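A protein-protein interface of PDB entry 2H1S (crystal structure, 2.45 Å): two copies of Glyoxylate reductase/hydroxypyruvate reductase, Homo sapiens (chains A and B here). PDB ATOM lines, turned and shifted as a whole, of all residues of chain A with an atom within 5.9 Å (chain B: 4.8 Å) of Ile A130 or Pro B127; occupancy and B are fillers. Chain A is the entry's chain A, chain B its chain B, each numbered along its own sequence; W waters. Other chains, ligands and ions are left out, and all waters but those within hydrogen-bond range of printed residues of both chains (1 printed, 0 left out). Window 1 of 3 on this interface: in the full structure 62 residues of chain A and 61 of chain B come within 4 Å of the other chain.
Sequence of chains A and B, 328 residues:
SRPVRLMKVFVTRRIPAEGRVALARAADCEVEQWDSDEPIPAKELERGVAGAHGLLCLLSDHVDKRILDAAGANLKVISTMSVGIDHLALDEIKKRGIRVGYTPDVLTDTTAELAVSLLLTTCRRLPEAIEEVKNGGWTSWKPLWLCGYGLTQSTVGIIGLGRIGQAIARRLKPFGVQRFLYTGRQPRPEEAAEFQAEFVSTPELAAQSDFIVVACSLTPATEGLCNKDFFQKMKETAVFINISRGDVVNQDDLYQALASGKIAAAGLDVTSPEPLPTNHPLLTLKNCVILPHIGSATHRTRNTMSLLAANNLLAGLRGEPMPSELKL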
ATOM      1  N   ARG A 125      15.189  27.283  20.361  1.00  0.00           N
ATOM      2  CA  ARG A 125      14.842  26.454  19.176  1.00  0.00           C
ATOM      3  C   ARG A 125      13.336  26.351  18.870  1.00  0.00           C
ATOM      4  O   ARG A 125      12.848  25.287  18.398  1.00  0.00           O
ATOM      5  CB  ARG A 125      15.422  25.061  19.329  1.00  0.00           C
ATOM      6  CG  ARG A 125      16.919  25.081  19.584  1.00  0.00           C
ATOM      7  CD  ARG A 125      17.434  23.708  19.851  1.00  0.00           C
ATOM      8  NE  ARG A 125      17.283  22.895  18.659  1.00  0.00           N
ATOM      9  CZ  ARG A 125      17.603  21.615  18.576  1.00  0.00           C
ATOM     10  NH1 ARG A 125      18.076  20.957  19.635  1.00  0.00           N
ATOM     11  NH2 ARG A 125      17.425  20.982  17.432  1.00  0.00           N
ATOM     12  N   LEU A 126      12.612  27.448  19.129  1.00  0.00           N
ATOM     13  CA  LEU A 126      11.177  27.505  18.871  1.00  0.00           C
ATOM     14  C   LEU A 126      10.806  27.146  17.418  1.00  0.00           C
ATOM     15  O   LEU A 126       9.974  26.252  17.200  1.00  0.00           O
ATOM     16  CB  LEU A 126      10.568  28.844  19.315  1.00  0.00           C
ATOM     17  CG  LEU A 126      10.152  28.952  20.812  1.00  0.00           C
ATOM     18  CD1 LEU A 126      11.263  28.485  21.773  1.00  0.00           C
ATOM     19  CD2 LEU A 126       9.749  30.360  21.141  1.00  0.00           C
ATOM     20  N   PRO A 127      11.468  27.776  16.414  1.00  0.00           N
ATOM     21  CA  PRO A 127      11.099  27.424  15.027  1.00  0.00           C
ATOM     22  C   PRO A 127      11.143  25.927  14.727  1.00  0.00           C
ATOM     23  O   PRO A 127      10.155  25.395  14.224  1.00  0.00           O
ATOM     24  CB  PRO A 127      12.135  28.166  14.197  1.00  0.00           C
ATOM     25  CG  PRO A 127      12.571  29.325  15.073  1.00  0.00           C
ATOM     26  CD  PRO A 127      12.548  28.781  16.460  1.00  0.00           C
ATOM     27  N   GLU A 128      12.234  25.225  15.058  1.00  0.00           N
ATOM     28  CA  GLU A 128      12.198  23.757  14.890  1.00  0.00           C
ATOM     29  C   GLU A 128      11.065  23.160  15.701  1.00  0.00           C
ATOM     30  O   GLU A 128      10.403  22.236  15.221  1.00  0.00           O
ATOM     31  CB  GLU A 128      13.509  23.013  15.207  1.00  0.00           C
ATOM     32  CG  GLU A 128      14.753  23.631  14.591  1.00  0.00           C
ATOM     33  CD  GLU A 128      16.051  23.024  15.100  1.00  0.00           C
ATOM     34  OE1 GLU A 128      16.436  21.944  14.615  1.00  0.00           O
ATOM     35  OE2 GLU A 128      16.702  23.657  15.950  1.00  0.00           O
ATOM     36  N   ALA A 129      10.836  23.671  16.912  1.00  0.00           N
ATOM     37  CA  ALA A 129       9.832  23.055  17.790  1.00  0.00           C
ATOM     38  C   ALA A 129       8.438  23.214  17.152  1.00  0.00           C
ATOM     39  O   ALA A 129       7.700  22.211  17.012  1.00  0.00           O
ATOM     40  CB  ALA A 129       9.924  23.601  19.180  1.00  0.00           C
ATOM     41  N   ILE A 130       8.130  24.433  16.689  1.00  0.00           N
ATOM     42  CA  ILE A 130       6.855  24.737  15.994  1.00  0.00           C
ATOM     43  C   ILE A 130       6.587  23.768  14.842  1.00  0.00           C
ATOM     44  O   ILE A 130       5.490  23.222  14.699  1.00  0.00           O
ATOM     45  CB  ILE A 130       6.842  26.165  15.412  1.00  0.00           C
ATOM     46  CG1 ILE A 130       6.861  27.191  16.556  1.00  0.00           C
ATOM     47  CG2 ILE A 130       5.601  26.371  14.493  1.00  0.00           C
ATOM     48  CD1 ILE A 130       7.047  28.676  16.143  1.00  0.00           C
ATOM     49  N   GLU A 131       7.618  23.550  14.031  1.00  0.00           N
ATOM     50  CA  GLU A 131       7.544  22.679  12.885  1.00  0.00           C
ATOM     51  C   GLU A 131       7.369  21.223  13.305  1.00  0.00           C
ATOM     52  O   GLU A 131       6.673  20.465  12.606  1.00  0.00           O
ATOM     53  CB  GLU A 131       8.773  22.889  11.976  1.00  0.00           C
ATOM     54  CG  GLU A 131       8.942  21.903  10.797  1.00  0.00           C
ATOM     55  CD  GLU A 131       7.867  22.034   9.698  1.00  0.00           C
ATOM     56  OE1 GLU A 131       7.068  22.988   9.723  1.00  0.00           O
ATOM     57  OE2 GLU A 131       7.834  21.177   8.784  1.00  0.00           O
ATOM     58  N   GLU A 132       7.960  20.810  14.441  1.00  0.00           N
ATOM     59  CA  GLU A 132       7.818  19.411  14.841  1.00  0.00           C
ATOM     60  C   GLU A 132       6.372  19.085  15.207  1.00  0.00           C
ATOM     61  O   GLU A 132       5.905  17.979  14.962  1.00  0.00           O
ATOM     62  CB  GLU A 132       8.768  19.027  15.955  1.00  0.00           C
ATOM     63  CG  GLU A 132      10.239  18.817  15.501  1.00  0.00           C
ATOM     64  CD  GLU A 132      10.398  17.884  14.320  1.00  0.00           C
ATOM     65  OE1 GLU A 132       9.885  16.748  14.377  1.00  0.00           O
ATOM     66  OE2 GLU A 132      11.064  18.282  13.336  1.00  0.00           O
ATOM     67  N   VAL A 133       5.673  20.089  15.731  1.00  0.00           N
ATOM     68  CA  VAL A 133       4.245  20.032  15.995  1.00  0.00           C
ATOM     69  C   VAL A 133       3.466  19.886  14.693  1.00  0.00           C
ATOM     70  O   VAL A 133       2.605  19.012  14.572  1.00  0.00           O
ATOM     71  CB  VAL A 133       3.737  21.334  16.632  1.00  0.00           C
ATOM     72  CG1 VAL A 133       2.197  21.270  16.757  1.00  0.00           C
ATOM     73  CG2 VAL A 133       4.402  21.573  17.957  1.00  0.00           C
ATOM     74  N   LYS A 134       3.749  20.779  13.743  1.00  0.00           N
ATOM     75  CA  LYS A 134       3.012  20.826  12.472  1.00  0.00           C
ATOM     76  C   LYS A 134       3.207  19.596  11.604  1.00  0.00           C
ATOM     77  O   LYS A 134       2.306  19.230  10.864  1.00  0.00           O
ATOM     78  CB  LYS A 134       3.404  22.070  11.665  1.00  0.00           C
ATOM     79  CG  LYS A 134       2.763  23.373  12.161  1.00  0.00           C
ATOM     80  CD  LYS A 134       3.301  24.556  11.404  1.00  0.00           C
ATOM     81  CE  LYS A 134       2.726  25.872  11.892  1.00  0.00           C
ATOM     82  NZ  LYS A 134       3.510  27.046  11.332  1.00  0.00           N
ATOM     83  N   ASN A 135       4.380  18.967  11.687  1.00  0.00           N
ATOM     84  CA  ASN A 135       4.768  17.936  10.722  1.00  0.00           C
ATOM     85  C   ASN A 135       4.684  16.518  11.247  1.00  0.00           C
ATOM     86  O   ASN A 135       5.077  15.602  10.551  1.00  0.00           O
ATOM     87  CB  ASN A 135       6.179  18.213  10.121  1.00  0.00           C
ATOM     88  CG  ASN A 135       7.327  17.816  11.065  1.00  0.00           C
ATOM     89  OD1 ASN A 135       7.134  17.109  12.043  1.00  0.00           O
ATOM     90  ND2 ASN A 135       8.512  18.284  10.770  1.00  0.00           N
ATOM     91  N   THR B 121       7.877  35.424  21.207  1.00  0.00           N
ATOM     92  CA  THR B 121       7.686  34.896  19.876  1.00  0.00           C
ATOM     93  C   THR B 121       6.276  35.090  19.419  1.00  0.00           C
ATOM     94  O   THR B 121       6.046  35.331  18.238  1.00  0.00           O
ATOM     95  CB  THR B 121       7.950  33.414  19.933  1.00  0.00           C
ATOM     96  OG1 THR B 121       9.346  33.222  20.004  1.00  0.00           O
ATOM     97  CG2 THR B 121       7.440  32.708  18.768  1.00  0.00           C
ATOM     98  N   ARG B 125       5.310  38.134  16.959  1.00  0.00           N
ATOM     99  CA  ARG B 125       4.873  37.536  15.668  1.00  0.00           C
ATOM    100  C   ARG B 125       5.993  36.906  14.884  1.00  0.00           C
ATOM    101  O   ARG B 125       6.005  36.851  13.624  1.00  0.00           O
ATOM    102  CB  ARG B 125       4.109  38.535  14.793  1.00  0.00           C
ATOM    103  CG  ARG B 125       2.846  39.030  15.434  1.00  0.00           C
ATOM    104  CD  ARG B 125       2.281  40.223  14.667  1.00  0.00           C
ATOM    105  NE  ARG B 125       1.518  39.793  13.504  1.00  0.00           N
ATOM    106  CZ  ARG B 125       0.909  40.612  12.643  1.00  0.00           C
ATOM    107  NH1 ARG B 125       0.976  41.934  12.787  1.00  0.00           N
ATOM    108  NH2 ARG B 125       0.267  40.099  11.609  1.00  0.00           N
ATOM    109  N   LEU B 126       6.925  36.345  15.635  1.00  0.00           N
ATOM    110  CA  LEU B 126       8.102  35.780  14.990  1.00  0.00           C
ATOM    111  C   LEU B 126       7.773  34.687  13.960  1.00  0.00           C
ATOM    112  O   LEU B 126       8.246  34.743  12.843  1.00  0.00           O
ATOM    113  CB  LEU B 126       9.148  35.409  16.036  1.00  0.00           C
ATOM    114  CG  LEU B 126      10.088  36.587  16.326  1.00  0.00           C
ATOM    115  CD1 LEU B 126       9.361  37.757  16.884  1.00  0.00           C
ATOM    116  CD2 LEU B 126      11.258  36.179  17.270  1.00  0.00           C
ATOM    117  N   PRO B 127       6.896  33.747  14.299  1.00  0.00           N
ATOM    118  CA  PRO B 127       6.604  32.698  13.293  1.00  0.00           C
ATOM    119  C   PRO B 127       6.029  33.225  11.976  1.00  0.00           C
ATOM    120  O   PRO B 127       6.530  32.869  10.924  1.00  0.00           O
ATOM    121  CB  PRO B 127       5.626  31.754  14.010  1.00  0.00           C
ATOM    122  CG  PRO B 127       5.867  32.057  15.482  1.00  0.00           C
ATOM    123  CD  PRO B 127       6.152  33.543  15.545  1.00  0.00           C
ATOM    124  N   GLU B 128       5.011  34.068  12.025  1.00  0.00           N
ATOM    125  CA  GLU B 128       4.551  34.755  10.833  1.00  0.00           C
ATOM    126  C   GLU B 128       5.760  35.396  10.136  1.00  0.00           C
ATOM    127  O   GLU B 128       5.915  35.246   8.916  1.00  0.00           O
ATOM    128  CB  GLU B 128       3.488  35.803  11.183  1.00  0.00           C
ATOM    129  CG  GLU B 128       2.161  35.212  11.610  1.00  0.00           C
ATOM    130  CD  GLU B 128       1.207  36.255  12.177  1.00  0.00           C
ATOM    131  OE1 GLU B 128       1.453  36.821  13.279  1.00  0.00           O
ATOM    132  OE2 GLU B 128       0.207  36.519  11.491  1.00  0.00           O
ATOM    133  N   ALA B 129       6.622  36.078  10.903  1.00  0.00           N
ATOM    134  CA  ALA B 129       7.737  36.797  10.302  1.00  0.00           C
ATOM    135  C   ALA B 129       8.658  35.831   9.585  1.00  0.00           C
ATOM    136  O   ALA B 129       9.049  36.054   8.434  1.00  0.00           O
ATOM    137  CB  ALA B 129       8.501  37.574  11.310  1.00  0.00           C
ATOM    138  N   ILE B 130       9.005  34.743  10.262  1.00  0.00           N
ATOM    139  CA  ILE B 130       9.852  33.745   9.663  1.00  0.00           C
ATOM    140  C   ILE B 130       9.271  33.215   8.349  1.00  0.00           C
ATOM    141  O   ILE B 130       9.997  33.120   7.361  1.00  0.00           O
ATOM    142  CB  ILE B 130      10.181  32.579  10.665  1.00  0.00           C
ATOM    143  CG1 ILE B 130      11.069  33.113  11.778  1.00  0.00           C
ATOM    144  CG2 ILE B 130      10.910  31.422   9.941  1.00  0.00           C
ATOM    145  CD1 ILE B 130      10.887  32.469  13.089  1.00  0.00           C
ATOM    146  N   GLU B 131       7.982  32.891   8.314  1.00  0.00           N
ATOM    147  CA  GLU B 131       7.402  32.364   7.088  1.00  0.00           C
ATOM    148  C   GLU B 131       7.326  33.420   5.991  1.00  0.00           C
ATOM    149  O   GLU B 131       7.407  33.061   4.816  1.00  0.00           O
ATOM    150  CB  GLU B 131       6.034  31.756   7.337  1.00  0.00           C
ATOM    151  CG  GLU B 131       5.276  31.186   6.086  1.00  0.00           C
ATOM    152  CD  GLU B 131       5.855  29.861   5.553  1.00  0.00           C
ATOM    153  OE1 GLU B 131       6.747  29.304   6.236  1.00  0.00           O
ATOM    154  OE2 GLU B 131       5.421  29.375   4.463  1.00  0.00           O
ATOM    155  N   VAL B 289       0.519  30.026  18.624  1.00  0.00           N
ATOM    156  CA  VAL B 289       1.814  29.342  18.586  1.00  0.00           C
ATOM    157  C   VAL B 289       1.738  28.153  19.523  1.00  0.00           C
ATOM    158  O   VAL B 289       1.334  28.304  20.694  1.00  0.00           O
ATOM    159  CB  VAL B 289       2.932  30.300  19.018  1.00  0.00           C
ATOM    160  CG1 VAL B 289       4.289  29.622  19.058  1.00  0.00           C
ATOM    161  CG2 VAL B 289       2.927  31.514  18.093  1.00  0.00           C
ATOM    162  N   ILE B 290       2.092  26.974  18.997  1.00  0.00           N
ATOM    163  CA  ILE B 290       2.145  25.791  19.814  1.00  0.00           C
ATOM    164  C   ILE B 290       3.538  25.144  19.793  1.00  0.00           C
ATOM    165  O   ILE B 290       4.051  24.759  18.718  1.00  0.00           O
ATOM    166  CB  ILE B 290       1.112  24.775  19.352  1.00  0.00           C
ATOM    167  CG1 ILE B 290      -0.308  25.358  19.537  1.00  0.00           C
ATOM    168  CG2 ILE B 290       1.308  23.491  20.122  1.00  0.00           C
ATOM    169  CD1 ILE B 290      -1.344  24.715  18.706  1.00  0.00           C
ATOM    170  N   LEU B 291       4.159  25.042  20.972  1.00  0.00           N
ATOM    171  CA  LEU B 291       5.385  24.251  21.141  1.00  0.00           C
ATOM    172  C   LEU B 291       5.055  22.890  21.759  1.00  0.00           C
ATOM    173  O   LEU B 291       4.053  22.753  22.459  1.00  0.00           O
ATOM    174  CB  LEU B 291       6.410  24.964  22.027  1.00  0.00           C
ATOM    175  CG  LEU B 291       6.503  26.465  21.814  1.00  0.00           C
ATOM    176  CD1 LEU B 291       7.254  27.040  23.030  1.00  0.00           C
ATOM    177  CD2 LEU B 291       7.114  26.846  20.453  1.00  0.00           C
HETATM  178  O   HOH W   1       3.289  24.622  16.094  1.00  0.00           O
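The backbone NH (N) of Leu B126 lies within hydrogen-bond range of the backbone carbonyl oxygen (O) of Thr B121 (2.9 Å).
Among the printed residues, pairs that only touch across the chains: Leu A126 with Thr B121, Val A133 with Ile B290, Ile A130 with Pro B127, Leu A126 with Leu B291, Ile A130 with Ile B290 and Ile A130 with Leu B291.
Of chain B, only Pro B127 (3.6 Å), Ile B290 (3.9 Å) and Leu B291 (3.9 Å) come within 4 Å of Ile A130.
Of the printed residues of chain B, Val A133 touches Ile B290 (3.3 Å).
Lys A134 touches none of the printed residues of chain B.
Of chain A, only Ile A130 comes within 4 Å of Pro B127.
Of the printed residues of chain A, Leu B291 touches Leu A126 and Ile A130.
The nearest residue of chain B that does not touch Ile A130 is Val B289 (4.1 Å).
Of the 11 printed residues of chain B, 4 touch a printed residue of chain A.
Hydrophobic or aromatic side chains of chain B within 4 Å of the printed part of chain A: Pro B127 and Leu B291.
Along chain B the printed residues that touch a printed residue of chain A span positions 121 to 291.
Among the printed residues, 6 pairs touch across the chains.
Ile A130 touches Pro B127, but with the chains exchanged Pro A127 does not touch Ile B130 (4.1 Å).
Of the 6 pairs that touch across the chains among the printed residues, none has its exchanged pair printed and touching as well.
Water W1 lies within hydrogen-bond range of the backbone carbonyl oxygen of Ile B290 (2.7 Å) and the backbone carbonyl oxygen of Ile A130 (3.0 Å).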
